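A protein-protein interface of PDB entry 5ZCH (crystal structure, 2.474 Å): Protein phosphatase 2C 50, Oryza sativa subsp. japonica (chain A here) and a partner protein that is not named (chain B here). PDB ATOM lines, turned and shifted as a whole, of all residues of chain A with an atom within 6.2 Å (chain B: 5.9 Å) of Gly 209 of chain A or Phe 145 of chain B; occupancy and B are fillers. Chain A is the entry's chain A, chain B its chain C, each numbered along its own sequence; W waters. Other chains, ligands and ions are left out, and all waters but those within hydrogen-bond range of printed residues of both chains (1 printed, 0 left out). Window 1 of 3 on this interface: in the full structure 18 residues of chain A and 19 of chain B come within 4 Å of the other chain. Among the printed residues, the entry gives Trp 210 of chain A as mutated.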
ATOM      1  N   LYS A 198       8.213  -6.917  15.116  1.00  0.00           N
ATOM      2  CA  LYS A 198       9.136  -6.766  14.001  1.00  0.00           C
ATOM      3  C   LYS A 198       8.874  -7.831  12.948  1.00  0.00           C
ATOM      4  O   LYS A 198       8.610  -8.993  13.273  1.00  0.00           O
ATOM      5  CB  LYS A 198      10.595  -6.848  14.468  1.00  0.00           C
ATOM      6  CG  LYS A 198      10.972  -5.806  15.507  1.00  0.00           C
ATOM      7  CD  LYS A 198      12.457  -5.857  15.824  1.00  0.00           C
ATOM      8  CE  LYS A 198      12.958  -4.518  16.338  1.00  0.00           C
ATOM      9  NZ  LYS A 198      14.168  -4.060  15.603  1.00  0.00           N
ATOM     10  N   VAL A 199       8.931  -7.420  11.685  1.00  0.00           N
ATOM     11  CA  VAL A 199       8.909  -8.329  10.546  1.00  0.00           C
ATOM     12  C   VAL A 199      10.319  -8.337   9.974  1.00  0.00           C
ATOM     13  O   VAL A 199      10.791  -7.318   9.455  1.00  0.00           O
ATOM     14  CB  VAL A 199       7.879  -7.905   9.491  1.00  0.00           C
ATOM     15  CG1 VAL A 199       7.936  -8.834   8.288  1.00  0.00           C
ATOM     16  CG2 VAL A 199       6.482  -7.885  10.090  1.00  0.00           C
ATOM     17  N   ILE A 200      10.999  -9.477  10.068  1.00  0.00           N
ATOM     18  CA  ILE A 200      12.424  -9.566   9.776  1.00  0.00           C
ATOM     19  C   ILE A 200      12.632 -10.520   8.609  1.00  0.00           C
ATOM     20  O   ILE A 200      12.147 -11.657   8.636  1.00  0.00           O
ATOM     21  CB  ILE A 200      13.222 -10.034  11.007  1.00  0.00           C
ATOM     22  CG1 ILE A 200      12.937  -9.127  12.207  1.00  0.00           C
ATOM     23  CG2 ILE A 200      14.711 -10.069  10.700  1.00  0.00           C
ATOM     24  CD1 ILE A 200      13.379  -9.711  13.530  1.00  0.00           C
ATOM     25  N   GLN A 201      13.354 -10.057   7.592  1.00  0.00           N
ATOM     26  CA  GLN A 201      13.780 -10.904   6.480  1.00  0.00           C
ATOM     27  C   GLN A 201      14.867 -11.847   6.979  1.00  0.00           C
ATOM     28  O   GLN A 201      16.031 -11.462   7.108  1.00  0.00           O
ATOM     29  CB  GLN A 201      14.270 -10.061   5.310  1.00  0.00           C
ATOM     30  CG  GLN A 201      14.629 -10.881   4.080  1.00  0.00           C
ATOM     31  CD  GLN A 201      14.965 -10.021   2.878  1.00  0.00           C
ATOM     32  OE1 GLN A 201      14.112  -9.757   2.032  1.00  0.00           O
ATOM     33  NE2 GLN A 201      16.215  -9.581   2.798  1.00  0.00           N
ATOM     34  N   TRP A 202      14.492 -13.093   7.263  1.00  0.00           N
ATOM     35  CA  TRP A 202      15.398 -14.081   7.856  1.00  0.00           C
ATOM     36  C   TRP A 202      15.034 -15.433   7.242  1.00  0.00           C
ATOM     37  O   TRP A 202      14.221 -16.177   7.798  1.00  0.00           O
ATOM     38  CB  TRP A 202      15.275 -14.091   9.376  1.00  0.00           C
ATOM     39  CG  TRP A 202      16.397 -14.779  10.089  1.00  0.00           C
ATOM     40  CD1 TRP A 202      16.648 -16.120  10.122  1.00  0.00           C
ATOM     41  CD2 TRP A 202      17.415 -14.160  10.885  1.00  0.00           C
ATOM     42  NE1 TRP A 202      17.762 -16.373  10.885  1.00  0.00           N
ATOM     43  CE2 TRP A 202      18.252 -15.187  11.365  1.00  0.00           C
ATOM     44  CE3 TRP A 202      17.701 -12.837  11.236  1.00  0.00           C
ATOM     45  CZ2 TRP A 202      19.355 -14.933  12.178  1.00  0.00           C
ATOM     46  CZ3 TRP A 202      18.797 -12.587  12.042  1.00  0.00           C
ATOM     47  CH2 TRP A 202      19.609 -13.629  12.505  1.00  0.00           C
ATOM     48  N   GLY A 204      13.395 -15.535   4.338  1.00  0.00           N
ATOM     49  CA  GLY A 204      12.020 -15.131   4.132  1.00  0.00           C
ATOM     50  C   GLY A 204      11.549 -14.179   5.214  1.00  0.00           C
ATOM     51  O   GLY A 204      12.054 -14.174   6.344  1.00  0.00           O
ATOM     52  N   ARG A 206       9.561 -12.880   8.177  1.00  0.00           N
ATOM     53  CA  ARG A 206       9.032 -13.658   9.285  1.00  0.00           C
ATOM     54  C   ARG A 206       8.691 -12.747  10.455  1.00  0.00           C
ATOM     55  O   ARG A 206       9.361 -11.739  10.697  1.00  0.00           O
ATOM     56  CB  ARG A 206      10.029 -14.731   9.743  1.00  0.00           C
ATOM     57  CG  ARG A 206      10.123 -15.932   8.817  1.00  0.00           C
ATOM     58  CD  ARG A 206      11.394 -16.725   9.073  1.00  0.00           C
ATOM     59  NE  ARG A 206      11.650 -17.701   8.019  1.00  0.00           N
ATOM     60  CZ  ARG A 206      11.190 -18.949   8.028  1.00  0.00           C
ATOM     61  NH1 ARG A 206      10.448 -19.377   9.041  1.00  0.00           N
ATOM     62  NH2 ARG A 206      11.472 -19.769   7.025  1.00  0.00           N
ATOM     63  N   VAL A 207       7.636 -13.120  11.178  1.00  0.00           N
ATOM     64  CA  VAL A 207       7.282 -12.437  12.419  1.00  0.00           C
ATOM     65  C   VAL A 207       8.364 -12.721  13.451  1.00  0.00           C
ATOM     66  O   VAL A 207       8.636 -13.881  13.780  1.00  0.00           O
ATOM     67  CB  VAL A 207       5.903 -12.888  12.919  1.00  0.00           C
ATOM     68  CG1 VAL A 207       5.527 -12.133  14.186  1.00  0.00           C
ATOM     69  CG2 VAL A 207       4.853 -12.688  11.838  1.00  0.00           C
ATOM     70  N   SER A 208       8.991 -11.659  13.960  1.00  0.00           N
ATOM     71  CA  SER A 208      10.099 -11.754  14.910  1.00  0.00           C
ATOM     72  C   SER A 208      11.273 -12.547  14.348  1.00  0.00           C
ATOM     73  O   SER A 208      12.111 -13.046  15.108  1.00  0.00           O
ATOM     74  CB  SER A 208       9.642 -12.362  16.243  1.00  0.00           C
ATOM     75  OG  SER A 208       8.508 -11.684  16.752  1.00  0.00           O
ATOM     76  N   GLY A 209      11.354 -12.676  13.025  1.00  0.00           N
ATOM     77  CA  GLY A 209      12.349 -13.523  12.404  1.00  0.00           C
ATOM     78  C   GLY A 209      12.059 -15.002  12.491  1.00  0.00           C
ATOM     79  O   GLY A 209      12.918 -15.809  12.117  1.00  0.00           O
ATOM     80  N   TRP A 210      10.869 -15.384  12.955  1.00  0.00           N
ATOM     81  CA  TRP A 210      10.547 -16.776  13.257  1.00  0.00           C
ATOM     82  C   TRP A 210       9.490 -17.315  12.309  1.00  0.00           C
ATOM     83  O   TRP A 210       9.793 -18.161  11.462  1.00  0.00           O
ATOM     84  CB  TRP A 210      10.114 -16.866  14.729  1.00  0.00           C
ATOM     85  CG  TRP A 210       9.463 -18.153  15.217  1.00  0.00           C
ATOM     86  CD1 TRP A 210       9.043 -19.223  14.472  1.00  0.00           C
ATOM     87  CD2 TRP A 210       9.157 -18.476  16.578  1.00  0.00           C
ATOM     88  NE1 TRP A 210       8.497 -20.184  15.285  1.00  0.00           N
ATOM     89  CE2 TRP A 210       8.556 -19.751  16.583  1.00  0.00           C
ATOM     90  CE3 TRP A 210       9.335 -17.811  17.794  1.00  0.00           C
ATOM     91  CZ2 TRP A 210       8.134 -20.372  17.756  1.00  0.00           C
ATOM     92  CZ3 TRP A 210       8.915 -18.429  18.958  1.00  0.00           C
ATOM     93  CH2 TRP A 210       8.320 -19.695  18.930  1.00  0.00           C
ATOM     94  N   LEU A 211       8.242 -16.861  12.419  1.00  0.00           N
ATOM     95  CA  LEU A 211       7.127 -17.485  11.719  1.00  0.00           C
ATOM     96  C   LEU A 211       6.907 -16.830  10.361  1.00  0.00           C
ATOM     97  O   LEU A 211       6.791 -15.604  10.266  1.00  0.00           O
ATOM     98  CB  LEU A 211       5.853 -17.399  12.558  1.00  0.00           C
ATOM     99  CG  LEU A 211       4.845 -18.529  12.348  1.00  0.00           C
ATOM    100  CD1 LEU A 211       5.426 -19.857  12.812  1.00  0.00           C
ATOM    101  CD2 LEU A 211       3.539 -18.226  13.070  1.00  0.00           C
ATOM    102  N   PRO B  74      13.251 -20.890  10.905  1.00  0.00           N
ATOM    103  CA  PRO B  74      14.111 -20.615   9.739  1.00  0.00           C
ATOM    104  C   PRO B  74      15.136 -21.701   9.463  1.00  0.00           C
ATOM    105  O   PRO B  74      15.680 -21.741   8.353  1.00  0.00           O
ATOM    106  CB  PRO B  74      14.795 -19.290  10.107  1.00  0.00           C
ATOM    107  CG  PRO B  74      13.919 -18.679  11.143  1.00  0.00           C
ATOM    108  CD  PRO B  74      13.335 -19.820  11.914  1.00  0.00           C
ATOM    109  N   LEU B 103      22.996 -18.257  12.290  1.00  0.00           N
ATOM    110  CA  LEU B 103      23.660 -17.791  13.505  1.00  0.00           C
ATOM    111  C   LEU B 103      25.086 -18.338  13.497  1.00  0.00           C
ATOM    112  O   LEU B 103      25.396 -19.341  14.141  1.00  0.00           O
ATOM    113  CB  LEU B 103      22.888 -18.232  14.755  1.00  0.00           C
ATOM    114  CG  LEU B 103      21.491 -17.637  14.944  1.00  0.00           C
ATOM    115  CD1 LEU B 103      20.885 -18.100  16.260  1.00  0.00           C
ATOM    116  CD2 LEU B 103      21.540 -16.118  14.878  1.00  0.00           C
ATOM    117  N   ASP B 140      19.973  -5.069  15.742  1.00  0.00           N
ATOM    118  CA  ASP B 140      18.764  -5.146  16.551  1.00  0.00           C
ATOM    119  C   ASP B 140      17.774  -6.159  15.997  1.00  0.00           C
ATOM    120  O   ASP B 140      16.978  -6.718  16.761  1.00  0.00           O
ATOM    121  CB  ASP B 140      18.114  -3.768  16.660  1.00  0.00           C
ATOM    122  CG  ASP B 140      19.128  -2.664  16.883  1.00  0.00           C
ATOM    123  OD1 ASP B 140      19.882  -2.741  17.880  1.00  0.00           O
ATOM    124  OD2 ASP B 140      19.177  -1.723  16.065  1.00  0.00           O
ATOM    125  N   GLU B 141      17.807  -6.415  14.687  1.00  0.00           N
ATOM    126  CA  GLU B 141      17.022  -7.513  14.135  1.00  0.00           C
ATOM    127  C   GLU B 141      17.546  -8.852  14.639  1.00  0.00           C
ATOM    128  O   GLU B 141      16.772  -9.711  15.079  1.00  0.00           O
ATOM    129  CB  GLU B 141      17.054  -7.468  12.609  1.00  0.00           C
ATOM    130  CG  GLU B 141      16.118  -6.451  11.984  1.00  0.00           C
ATOM    131  CD  GLU B 141      16.151  -6.498  10.470  1.00  0.00           C
ATOM    132  OE1 GLU B 141      17.230  -6.784   9.910  1.00  0.00           O
ATOM    133  OE2 GLU B 141      15.101  -6.249   9.840  1.00  0.00           O
ATOM    134  N   THR B 142      18.866  -9.041  14.578  1.00  0.00           N
ATOM    135  CA  THR B 142      19.473 -10.276  15.064  1.00  0.00           C
ATOM    136  C   THR B 142      19.238 -10.447  16.560  1.00  0.00           C
ATOM    137  O   THR B 142      18.887 -11.538  17.025  1.00  0.00           O
ATOM    138  CB  THR B 142      20.969 -10.282  14.749  1.00  0.00           C
ATOM    139  OG1 THR B 142      21.168  -9.998  13.359  1.00  0.00           O
ATOM    140  CG2 THR B 142      21.584 -11.636  15.078  1.00  0.00           C
ATOM    141  N   CYS B 143      19.437  -9.375  17.331  1.00  0.00           N
ATOM    142  CA  CYS B 143      19.211  -9.447  18.772  1.00  0.00           C
ATOM    143  C   CYS B 143      17.753  -9.746  19.088  1.00  0.00           C
ATOM    144  O   CYS B 143      17.455 -10.536  19.992  1.00  0.00           O
ATOM    145  CB  CYS B 143      19.647  -8.143  19.440  1.00  0.00           C
ATOM    146  SG  CYS B 143      21.425  -8.005  19.720  1.00  0.00           S
ATOM    147  N   TYR B 144      16.826  -9.120  18.356  1.00  0.00           N
ATOM    148  CA  TYR B 144      15.408  -9.394  18.564  1.00  0.00           C
ATOM    149  C   TYR B 144      15.080 -10.853  18.281  1.00  0.00           C
ATOM    150  O   TYR B 144      14.315 -11.482  19.021  1.00  0.00           O
ATOM    151  CB  TYR B 144      14.561  -8.472  17.685  1.00  0.00           C
ATOM    152  CG  TYR B 144      13.083  -8.491  17.999  1.00  0.00           C
ATOM    153  CD1 TYR B 144      12.229  -9.382  17.358  1.00  0.00           C
ATOM    154  CD2 TYR B 144      12.538  -7.615  18.928  1.00  0.00           C
ATOM    155  CE1 TYR B 144      10.877  -9.402  17.639  1.00  0.00           C
ATOM    156  CE2 TYR B 144      11.185  -7.627  19.215  1.00  0.00           C
ATOM    157  CZ  TYR B 144      10.361  -8.523  18.566  1.00  0.00           C
ATOM    158  OH  TYR B 144       9.013  -8.542  18.846  1.00  0.00           O
ATOM    159  N   PHE B 145      15.655 -11.411  17.212  1.00  0.00           N
ATOM    160  CA  PHE B 145      15.378 -12.800  16.859  1.00  0.00           C
ATOM    161  C   PHE B 145      15.901 -13.756  17.925  1.00  0.00           C
ATOM    162  O   PHE B 145      15.178 -14.652  18.377  1.00  0.00           O
ATOM    163  CB  PHE B 145      15.989 -13.124  15.496  1.00  0.00           C
ATOM    164  CG  PHE B 145      15.865 -14.569  15.104  1.00  0.00           C
ATOM    165  CD1 PHE B 145      14.623 -15.174  15.024  1.00  0.00           C
ATOM    166  CD2 PHE B 145      16.992 -15.321  14.818  1.00  0.00           C
ATOM    167  CE1 PHE B 145      14.506 -16.504  14.667  1.00  0.00           C
ATOM    168  CE2 PHE B 145      16.881 -16.651  14.457  1.00  0.00           C
ATOM    169  CZ  PHE B 145      15.636 -17.243  14.380  1.00  0.00           C
ATOM    170  N   VAL B 146      17.157 -13.580  18.340  1.00  0.00           N
ATOM    171  CA  VAL B 146      17.743 -14.480  19.329  1.00  0.00           C
ATOM    172  C   VAL B 146      17.055 -14.319  20.680  1.00  0.00           C
ATOM    173  O   VAL B 146      16.812 -15.304  21.388  1.00  0.00           O
ATOM    174  CB  VAL B 146      19.261 -14.243  19.429  1.00  0.00           C
ATOM    175  CG1 VAL B 146      19.868 -15.129  20.507  1.00  0.00           C
ATOM    176  CG2 VAL B 146      19.924 -14.506  18.087  1.00  0.00           C
ATOM    177  N   GLU B 147      16.721 -13.081  21.057  1.00  0.00           N
ATOM    178  CA  GLU B 147      16.061 -12.851  22.339  1.00  0.00           C
ATOM    179  C   GLU B 147      14.702 -13.537  22.391  1.00  0.00           C
ATOM    180  O   GLU B 147      14.310 -14.075  23.434  1.00  0.00           O
ATOM    181  CB  GLU B 147      15.909 -11.352  22.597  1.00  0.00           C
ATOM    182  CG  GLU B 147      17.137 -10.691  23.201  1.00  0.00           C
ATOM    183  CD  GLU B 147      17.056  -9.177  23.161  1.00  0.00           C
ATOM    184  OE1 GLU B 147      15.971  -8.629  23.446  1.00  0.00           O
ATOM    185  OE2 GLU B 147      18.077  -8.534  22.840  1.00  0.00           O
ATOM    186  N   ALA B 148      13.963 -13.519  21.279  1.00  0.00           N
ATOM    187  CA  ALA B 148      12.662 -14.179  21.245  1.00  0.00           C
ATOM    188  C   ALA B 148      12.796 -15.677  21.491  1.00  0.00           C
ATOM    189  O   ALA B 148      12.000 -16.266  22.231  1.00  0.00           O
ATOM    190  CB  ALA B 148      11.972 -13.914  19.907  1.00  0.00           C
ATOM    191  N   LEU B 149      13.803 -16.309  20.885  1.00  0.00           N
ATOM    192  CA  LEU B 149      14.001 -17.741  21.082  1.00  0.00           C
ATOM    193  C   LEU B 149      14.466 -18.047  22.501  1.00  0.00           C
ATOM    194  O   LEU B 149      14.024 -19.030  23.107  1.00  0.00           O
ATOM    195  CB  LEU B 149      15.006 -18.277  20.063  1.00  0.00           C
ATOM    196  CG  LEU B 149      14.602 -18.179  18.591  1.00  0.00           C
ATOM    197  CD1 LEU B 149      15.748 -18.615  17.693  1.00  0.00           C
ATOM    198  CD2 LEU B 149      13.359 -19.008  18.318  1.00  0.00           C
ATOM    199  N   LEU B 150      15.355 -17.214  23.049  1.00  0.00           N
ATOM    200  CA  LEU B 150      15.884 -17.474  24.385  1.00  0.00           C
ATOM    201  C   LEU B 150      14.812 -17.296  25.453  1.00  0.00           C
ATOM    202  O   LEU B 150      14.757 -18.068  26.418  1.00  0.00           O
ATOM    203  CB  LEU B 150      17.077 -16.559  24.662  1.00  0.00           C
ATOM    204  CG  LEU B 150      18.320 -16.809  23.807  1.00  0.00           C
ATOM    205  CD1 LEU B 150      19.486 -15.961  24.288  1.00  0.00           C
ATOM    206  CD2 LEU B 150      18.685 -18.284  23.817  1.00  0.00           C
HETATM  207  O   HOH W   1      14.399  -7.610   7.574  1.00  0.00           O
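O of Trp 202 of chain A sits at hydrogen-bond distance from NE of Arg 206 of chain A (3.0 Å). The backbone NH (N) of Ser 208 of chain A lies within hydrogen-bond range of the backbone carbonyl oxygen (O) of Lys 198 of chain A (2.8 Å). The backbone NH (N) of Ile 200 of chain A sits at hydrogen-bond distance from the backbone carbonyl oxygen (O) of Arg 206 of chain A, at 2.9 Å. The guanidinium group (NH1) of Arg 206 of chain A lies within hydrogen-bond range of the backbone carbonyl oxygen (O) of Trp 210 of chain A (2.8 Å).
CD1 of Ile 200 of chain A touches O of Glu 141 of chain B (3.7 Å). CB of Pro 74 of chain B touches CD1 of Trp 202 of chain A, at 3.7 Å. Trp 202 of chain A touches Leu 103 of chain B (CZ2 to CD2, 3.7 Å). Thr 142 of chain B touches Trp 202 of chain A. Trp 202 of chain A touches Phe 145 of chain B. Arg 206 of chain A touches Pro 74 of chain B (NH1 to N, 3.7 Å). Ser 208 of chain A touches Tyr 144 of chain B (OG to CE1, 3.4 Å). Ser 208 of chain A touches Phe 145 of chain B (O to CD1, 3.3 Å). CE1 of Phe 145 of chain B touches O of Gly 209 of chain A (3.1 Å). Pro 74 of chain B touches Trp 210 of chain A (CD to O, 3.9 Å).
Of the printed residues of chain B, Ile 200 of chain A touches Glu 141 (3.7 Å). Gly 209 of chain A touches just these residues of chain B: Pro 74 (3.2 Å) and Phe 145 (3.1 Å). Of the printed residues of chain B, Trp 210 of chain A touches Pro 74 (3.9 Å). Printed residues of chain A within 4 Å of Pro 74 of chain B: Trp 202 (3.7 Å), Arg 206 (3.7 Å), Gly 209 (3.2 Å) and Trp 210 (3.9 Å). Printed residues of chain A within 4 Å of Leu 103 of chain B: Trp 202 (3.7 Å). Cys 143 of chain B touches none of the printed residues of chain A. Of the printed residues of chain A, Tyr 144 of chain B touches Lys 198 (3.5 Å) and Ser 208 (3.4 Å). Of chain A, only Trp 202, Ser 208 and Gly 209 come within 4 Å of Phe 145 of chain B. The nearest residue of chain B that does not touch Gly 209 of chain A is Tyr 144 of chain B (5.5 Å).
Of the 13 printed residues of chain B, 6 touch a printed residue of chain A. Hydrophobic or aromatic side chains of chain B that line the printed part of chain A: Pro 74, Leu 103, Tyr 144 and Phe 145. Hydrophobic or aromatic side chains of chain A within 4 Å of the printed part of chain B: Ile 200 and Trp 202. Along chain A the printed residues that touch a printed residue of chain B span positions 198 to 210. Among the printed residues, no Asp or Glu carboxylate lies within 4 Å of a Lys or Arg side-chain nitrogen of the other chain.
Water W1 lies within hydrogen-bond range of N of Gln 201 of chain A (2.7 Å) and OE2 of Glu 141 of chain B (2.7 Å).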
